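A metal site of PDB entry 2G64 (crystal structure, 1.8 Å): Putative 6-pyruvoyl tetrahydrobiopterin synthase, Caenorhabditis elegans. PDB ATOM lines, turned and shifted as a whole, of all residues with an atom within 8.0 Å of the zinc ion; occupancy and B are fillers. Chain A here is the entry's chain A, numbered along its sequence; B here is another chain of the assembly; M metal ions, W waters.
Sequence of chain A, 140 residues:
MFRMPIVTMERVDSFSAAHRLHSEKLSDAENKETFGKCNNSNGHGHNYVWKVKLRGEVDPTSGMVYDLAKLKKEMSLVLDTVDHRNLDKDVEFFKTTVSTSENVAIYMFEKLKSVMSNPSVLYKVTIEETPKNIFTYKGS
Water W1 lies within hydrogen-bond range of a ring nitrogen (NE2) of His 84 of chain B (2.9 Å) and the side-chain sulfur (SG) of Cys 38 (3.4 Å).
Three residues have an atom within 4 Å of the zinc ion: His 19, His 44 and His 46.
The nearest printed residue that does not touch the zinc ion is Cys 38 (4.5 Å).
Water W2 is bound to the zinc ion.
NE2 of His 46 is bound to the zinc ion (2.1 Å).
A ring nitrogen (NE2) of His 19 binds the zinc ion (2.1 Å).
NE2 of His 44 binds the zinc ion, at 2.1 Å.
Slightly farther from the zinc ion lies water W1 (2.7 Å).
A ring nitrogen (ND1) of His 46 lies close to the backbone carbonyl oxygen (O) of Glu 129, 3.4 Å away.
The backbone NH of His 46 is in hydrogen-bond range of the backbone carbonyl oxygen of Ala 17, at 3.0 Å.
OD1 of Asn 47 of chain B lies within hydrogen-bond range of ND1 of His 46 (2.9 Å).
A ring nitrogen (ND1) of His 19 lies within hydrogen-bond range of the side-chain hydroxyl (OG) of Ser 99.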
ATOM      1  N   ALA A  17     -25.542   1.594  33.892  1.00  0.00           N
ATOM      2  CA  ALA A  17     -24.670   1.933  32.771  1.00  0.00           C
ATOM      3  C   ALA A  17     -25.390   1.738  31.453  1.00  0.00           C
ATOM      4  O   ALA A  17     -26.324   0.924  31.329  1.00  0.00           O
ATOM      5  CB  ALA A  17     -23.379   1.097  32.805  1.00  0.00           C
ATOM      6  N   ALA A  18     -24.943   2.490  30.447  1.00  0.00           N
ATOM      7  CA  ALA A  18     -25.372   2.283  29.085  1.00  0.00           C
ATOM      8  C   ALA A  18     -24.361   1.398  28.347  1.00  0.00           C
ATOM      9  O   ALA A  18     -23.165   1.400  28.674  1.00  0.00           O
ATOM     10  CB  ALA A  18     -25.489   3.661  28.352  1.00  0.00           C
ATOM     11  N   HIS A  19     -24.827   0.684  27.345  1.00  0.00           N
ATOM     12  CA  HIS A  19     -23.906   0.030  26.419  1.00  0.00           C
ATOM     13  C   HIS A  19     -24.574  -0.286  25.090  1.00  0.00           C
ATOM     14  O   HIS A  19     -25.801  -0.104  24.930  1.00  0.00           O
ATOM     15  CB  HIS A  19     -23.261  -1.222  27.072  1.00  0.00           C
ATOM     16  CG  HIS A  19     -24.119  -2.455  27.065  1.00  0.00           C
ATOM     17  ND1 HIS A  19     -23.582  -3.720  26.890  1.00  0.00           N
ATOM     18  CD2 HIS A  19     -25.441  -2.634  27.262  1.00  0.00           C
ATOM     19  CE1 HIS A  19     -24.546  -4.613  26.951  1.00  0.00           C
ATOM     20  NE2 HIS A  19     -25.691  -3.988  27.193  1.00  0.00           N
ATOM     21  N   ARG A  20     -23.760  -0.690  24.120  1.00  0.00           N
ATOM     22  CA  ARG A  20     -24.254  -1.230  22.865  1.00  0.00           C
ATOM     23  C   ARG A  20     -23.347  -2.413  22.515  1.00  0.00           C
ATOM     24  O   ARG A  20     -22.109  -2.298  22.608  1.00  0.00           O
ATOM     25  CB  ARG A  20     -24.177  -0.157  21.780  1.00  0.00           C
ATOM     26  CG  ARG A  20     -24.469  -0.720  20.383  1.00  0.00           C
ATOM     27  CD  ARG A  20     -24.065   0.283  19.300  1.00  0.00           C
ATOM     28  NE  ARG A  20     -24.598  -0.159  18.016  1.00  0.00           N
ATOM     29  CZ  ARG A  20     -24.023   0.079  16.834  1.00  0.00           C
ATOM     30  NH1 ARG A  20     -22.859   0.713  16.764  1.00  0.00           N
ATOM     31  NH2 ARG A  20     -24.619  -0.356  15.728  1.00  0.00           N
ATOM     32  N   LEU A  21     -23.937  -3.547  22.153  1.00  0.00           N
ATOM     33  CA  LEU A  21     -23.138  -4.711  21.772  1.00  0.00           C
ATOM     34  C   LEU A  21     -22.787  -4.561  20.287  1.00  0.00           C
ATOM     35  O   LEU A  21     -23.666  -4.562  19.418  1.00  0.00           O
ATOM     36  CB  LEU A  21     -23.905  -6.003  22.032  1.00  0.00           C
ATOM     37  CG  LEU A  21     -24.177  -6.249  23.526  1.00  0.00           C
ATOM     38  CD1 LEU A  21     -24.855  -7.605  23.675  1.00  0.00           C
ATOM     39  CD2 LEU A  21     -22.825  -6.197  24.295  1.00  0.00           C
ATOM     40  N   LYS A  37     -31.444  -6.623  18.735  1.00  0.00           N
ATOM     41  CA  LYS A  37     -31.796  -5.333  19.335  1.00  0.00           C
ATOM     42  C   LYS A  37     -30.679  -4.778  20.240  1.00  0.00           C
ATOM     43  O   LYS A  37     -30.590  -3.570  20.468  1.00  0.00           O
ATOM     44  CB  LYS A  37     -33.093  -5.454  20.143  1.00  0.00           C
ATOM     45  CG  LYS A  37     -34.347  -5.455  19.274  1.00  0.00           C
ATOM     46  CD  LYS A  37     -35.609  -5.425  20.149  1.00  0.00           C
ATOM     47  CE  LYS A  37     -36.883  -5.408  19.311  1.00  0.00           C
ATOM     48  NZ  LYS A  37     -37.298  -4.016  18.962  1.00  0.00           N
ATOM     49  N   CYS A  38     -29.821  -5.659  20.747  1.00  0.00           N
ATOM     50  CA  CYS A  38     -28.691  -5.195  21.548  1.00  0.00           C
ATOM     51  C   CYS A  38     -27.681  -4.353  20.755  1.00  0.00           C
ATOM     52  O   CYS A  38     -26.894  -3.607  21.337  1.00  0.00           O
ATOM     53  CB  CYS A  38     -27.997  -6.354  22.257  1.00  0.00           C
ATOM     54  SG  CYS A  38     -29.041  -7.138  23.517  1.00  0.00           S
ATOM     55  N   ASN A  39     -27.751  -4.430  19.429  1.00  0.00           N
ATOM     56  CA  ASN A  39     -26.902  -3.610  18.572  1.00  0.00           C
ATOM     57  C   ASN A  39     -27.521  -2.226  18.256  1.00  0.00           C
ATOM     58  O   ASN A  39     -26.957  -1.465  17.460  1.00  0.00           O
ATOM     59  CB  ASN A  39     -26.583  -4.410  17.299  1.00  0.00           C
ATOM     60  CG  ASN A  39     -25.588  -3.719  16.395  1.00  0.00           C
ATOM     61  OD1 ASN A  39     -25.946  -3.291  15.289  1.00  0.00           O
ATOM     62  ND2 ASN A  39     -24.335  -3.611  16.849  1.00  0.00           N
ATOM     63  N   GLY A  43     -27.702   2.605  21.586  1.00  0.00           N
ATOM     64  CA  GLY A  43     -27.469   1.878  22.819  1.00  0.00           C
ATOM     65  C   GLY A  43     -28.736   1.638  23.634  1.00  0.00           C
ATOM     66  O   GLY A  43     -29.874   1.930  23.207  1.00  0.00           O
ATOM     67  N   HIS A  44     -28.519   1.054  24.804  1.00  0.00           N
ATOM     68  CA  HIS A  44     -29.582   0.782  25.761  1.00  0.00           C
ATOM     69  C   HIS A  44     -28.813   0.652  27.076  1.00  0.00           C
ATOM     70  O   HIS A  44     -27.643   1.089  27.146  1.00  0.00           O
ATOM     71  CB  HIS A  44     -30.357  -0.518  25.403  1.00  0.00           C
ATOM     72  CG  HIS A  44     -29.512  -1.764  25.411  1.00  0.00           C
ATOM     73  ND1 HIS A  44     -28.612  -2.066  24.403  1.00  0.00           N
ATOM     74  CD2 HIS A  44     -29.411  -2.774  26.312  1.00  0.00           C
ATOM     75  CE1 HIS A  44     -28.001  -3.208  24.680  1.00  0.00           C
ATOM     76  NE2 HIS A  44     -28.469  -3.655  25.829  1.00  0.00           N
ATOM     77  N   GLY A  45     -29.436   0.092  28.106  1.00  0.00           N
ATOM     78  CA  GLY A  45     -28.793   0.138  29.419  1.00  0.00           C
ATOM     79  C   GLY A  45     -29.359  -0.839  30.420  1.00  0.00           C
ATOM     80  O   GLY A  45     -30.352  -1.503  30.159  1.00  0.00           O
ATOM     81  N   HIS A  46     -28.705  -0.923  31.570  1.00  0.00           N
ATOM     82  CA  HIS A  46     -29.102  -1.895  32.597  1.00  0.00           C
ATOM     83  C   HIS A  46     -28.759  -1.313  33.954  1.00  0.00           C
ATOM     84  O   HIS A  46     -27.812  -0.529  34.075  1.00  0.00           O
ATOM     85  CB  HIS A  46     -28.354  -3.242  32.433  1.00  0.00           C
ATOM     86  CG  HIS A  46     -28.592  -3.923  31.126  1.00  0.00           C
ATOM     87  ND1 HIS A  46     -29.796  -4.482  30.790  1.00  0.00           N
ATOM     88  CD2 HIS A  46     -27.781  -4.103  30.053  1.00  0.00           C
ATOM     89  CE1 HIS A  46     -29.723  -4.990  29.567  1.00  0.00           C
ATOM     90  NE2 HIS A  46     -28.505  -4.767  29.098  1.00  0.00           N
ATOM     91  N   TYR A  48     -26.977  -3.042  36.654  1.00  0.00           N
ATOM     92  CA  TYR A  48     -26.253  -4.291  36.774  1.00  0.00           C
ATOM     93  C   TYR A  48     -26.128  -4.574  38.279  1.00  0.00           C
ATOM     94  O   TYR A  48     -25.720  -3.706  39.037  1.00  0.00           O
ATOM     95  CB  TYR A  48     -24.854  -4.118  36.186  1.00  0.00           C
ATOM     96  CG  TYR A  48     -24.771  -4.055  34.681  1.00  0.00           C
ATOM     97  CD1 TYR A  48     -24.632  -5.213  33.915  1.00  0.00           C
ATOM     98  CD2 TYR A  48     -24.771  -2.814  34.016  1.00  0.00           C
ATOM     99  CE1 TYR A  48     -24.519  -5.162  32.513  1.00  0.00           C
ATOM    100  CE2 TYR A  48     -24.647  -2.753  32.627  1.00  0.00           C
ATOM    101  CZ  TYR A  48     -24.536  -3.914  31.885  1.00  0.00           C
ATOM    102  OH  TYR A  48     -24.419  -3.836  30.533  1.00  0.00           O
ATOM    103  N   LEU A  87     -20.406   2.044  28.965  1.00  0.00           N
ATOM    104  CA  LEU A  87     -19.295   1.076  29.031  1.00  0.00           C
ATOM    105  C   LEU A  87     -18.362   1.179  27.816  1.00  0.00           C
ATOM    106  O   LEU A  87     -17.148   1.243  27.967  1.00  0.00           O
ATOM    107  CB  LEU A  87     -19.809  -0.356  29.197  1.00  0.00           C
ATOM    108  CG  LEU A  87     -20.690  -0.645  30.421  1.00  0.00           C
ATOM    109  CD1 LEU A  87     -20.989  -2.166  30.484  1.00  0.00           C
ATOM    110  CD2 LEU A  87     -19.975  -0.204  31.679  1.00  0.00           C
ATOM    111  N   SER A  99     -18.848  -5.504  25.169  1.00  0.00           N
ATOM    112  CA  SER A  99     -19.410  -5.342  26.516  1.00  0.00           C
ATOM    113  C   SER A  99     -20.587  -6.302  26.836  1.00  0.00           C
ATOM    114  O   SER A  99     -21.579  -5.916  27.487  1.00  0.00           O
ATOM    115  CB  SER A  99     -19.851  -3.878  26.705  1.00  0.00           C
ATOM    116  OG  SER A  99     -20.876  -3.547  25.765  1.00  0.00           O
ATOM    117  N   THR A 100     -20.489  -7.542  26.411  1.00  0.00           N
ATOM    118  CA  THR A 100     -21.459  -8.574  26.844  1.00  0.00           C
ATOM    119  C   THR A 100     -21.306  -8.732  28.337  1.00  0.00           C
ATOM    120  O   THR A 100     -20.249  -8.449  28.888  1.00  0.00           O
ATOM    121  CB  THR A 100     -21.168  -9.962  26.231  1.00  0.00           C
ATOM    122  OG1 THR A 100     -19.792 -10.319  26.462  1.00  0.00           O
ATOM    123  CG2 THR A 100     -21.456  -9.959  24.751  1.00  0.00           C
ATOM    124  N   SER A 101     -22.333  -9.225  29.018  1.00  0.00           N
ATOM    125  CA  SER A 101     -22.223  -9.366  30.473  1.00  0.00           C
ATOM    126  C   SER A 101     -21.173 -10.397  30.898  1.00  0.00           C
ATOM    127  O   SER A 101     -20.585 -10.285  31.970  1.00  0.00           O
ATOM    128  CB  SER A 101     -23.597  -9.652  31.097  1.00  0.00           C
ATOM    129  OG  SER A 101     -24.472  -8.569  30.835  1.00  0.00           O
ATOM    130  N   GLU A 129     -27.312  -8.891  34.668  1.00  0.00           N
ATOM    131  CA  GLU A 129     -27.612  -7.880  33.673  1.00  0.00           C
ATOM    132  C   GLU A 129     -29.070  -7.427  33.802  1.00  0.00           C
ATOM    133  O   GLU A 129     -29.363  -6.236  33.682  1.00  0.00           O
ATOM    134  CB  GLU A 129     -27.350  -8.521  32.327  1.00  0.00           C
ATOM    135  CG  GLU A 129     -27.814  -7.788  31.136  1.00  0.00           C
ATOM    136  CD  GLU A 129     -27.732  -8.716  29.937  1.00  0.00           C
ATOM    137  OE1 GLU A 129     -28.775  -9.231  29.517  1.00  0.00           O
ATOM    138  OE2 GLU A 129     -26.604  -8.979  29.485  1.00  0.00           O
ATOM    139  N   THR A 130     -29.955  -8.392  34.030  1.00  0.00           N
ATOM    140  CA  THR A 130     -31.318  -8.158  34.511  1.00  0.00           C
ATOM    141  C   THR A 130     -31.602  -9.259  35.530  1.00  0.00           C
ATOM    142  O   THR A 130     -30.793 -10.175  35.705  1.00  0.00           O
ATOM    143  CB  THR A 130     -32.369  -8.272  33.391  1.00  0.00           C
ATOM    144  OG1 THR A 130     -32.546  -9.643  33.072  1.00  0.00           O
ATOM    145  CG2 THR A 130     -31.933  -7.493  32.124  1.00  0.00           C
ATOM    146  N   ASN A 133     -31.116 -12.705  33.787  1.00  0.00           N
ATOM    147  CA  ASN A 133     -29.900 -13.047  33.017  1.00  0.00           C
ATOM    148  C   ASN A 133     -28.691 -12.845  33.934  1.00  0.00           C
ATOM    149  O   ASN A 133     -28.341 -11.701  34.241  1.00  0.00           O
ATOM    150  CB  ASN A 133     -29.733 -12.125  31.796  1.00  0.00           C
ATOM    151  CG  ASN A 133     -30.847 -12.293  30.765  1.00  0.00           C
ATOM    152  OD1 ASN A 133     -31.274 -13.406  30.481  1.00  0.00           O
ATOM    153  ND2 ASN A 133     -31.279 -11.188  30.170  1.00  0.00           N
ATOM    154  N   SER B  16     -35.358  -2.280  28.946  1.00  0.00           N
ATOM    155  CA  SER B  16     -34.000  -1.804  29.164  1.00  0.00           C
ATOM    156  C   SER B  16     -33.766  -0.608  28.247  1.00  0.00           C
ATOM    157  O   SER B  16     -34.098  -0.639  27.062  1.00  0.00           O
ATOM    158  CB  SER B  16     -33.006  -2.936  28.929  1.00  0.00           C
ATOM    159  OG  SER B  16     -33.176  -3.960  29.904  1.00  0.00           O
ATOM    160  N   ASN B  47     -32.639  -0.962  33.848  1.00  0.00           N
ATOM    161  CA  ASN B  47     -33.789  -1.837  33.600  1.00  0.00           C
ATOM    162  C   ASN B  47     -34.973  -1.205  34.309  1.00  0.00           C
ATOM    163  O   ASN B  47     -34.977  -1.105  35.529  1.00  0.00           O
ATOM    164  CB  ASN B  47     -33.548  -3.217  34.180  1.00  0.00           C
ATOM    165  CG  ASN B  47     -32.266  -3.831  33.690  1.00  0.00           C
ATOM    166  OD1 ASN B  47     -32.022  -3.905  32.484  1.00  0.00           O
ATOM    167  ND2 ASN B  47     -31.451  -4.308  34.623  1.00  0.00           N
ATOM    168  N   HIS B  84     -34.827  -1.601  24.716  1.00  0.00           N
ATOM    169  CA  HIS B  84     -33.542  -1.616  24.003  1.00  0.00           C
ATOM    170  C   HIS B  84     -33.299  -0.370  23.130  1.00  0.00           C
ATOM    171  O   HIS B  84     -32.658  -0.428  22.085  1.00  0.00           O
ATOM    172  CB  HIS B  84     -33.390  -2.908  23.222  1.00  0.00           C
ATOM    173  CG  HIS B  84     -33.028  -4.073  24.091  1.00  0.00           C
ATOM    174  ND1 HIS B  84     -33.961  -4.758  24.826  1.00  0.00           N
ATOM    175  CD2 HIS B  84     -31.828  -4.600  24.424  1.00  0.00           C
ATOM    176  CE1 HIS B  84     -33.363  -5.693  25.547  1.00  0.00           C
ATOM    177  NE2 HIS B  84     -32.067  -5.614  25.313  1.00  0.00           N
HETATM  178 ZN    ZN M   1     -27.567  -4.987  27.236  1.00  0.00          ZN
HETATM  179  O   HOH W   1     -29.765  -6.515  26.748  1.00  0.00           O
HETATM  180  O   HOH W   2     -27.368  -6.664  26.542  1.00  0.00           O
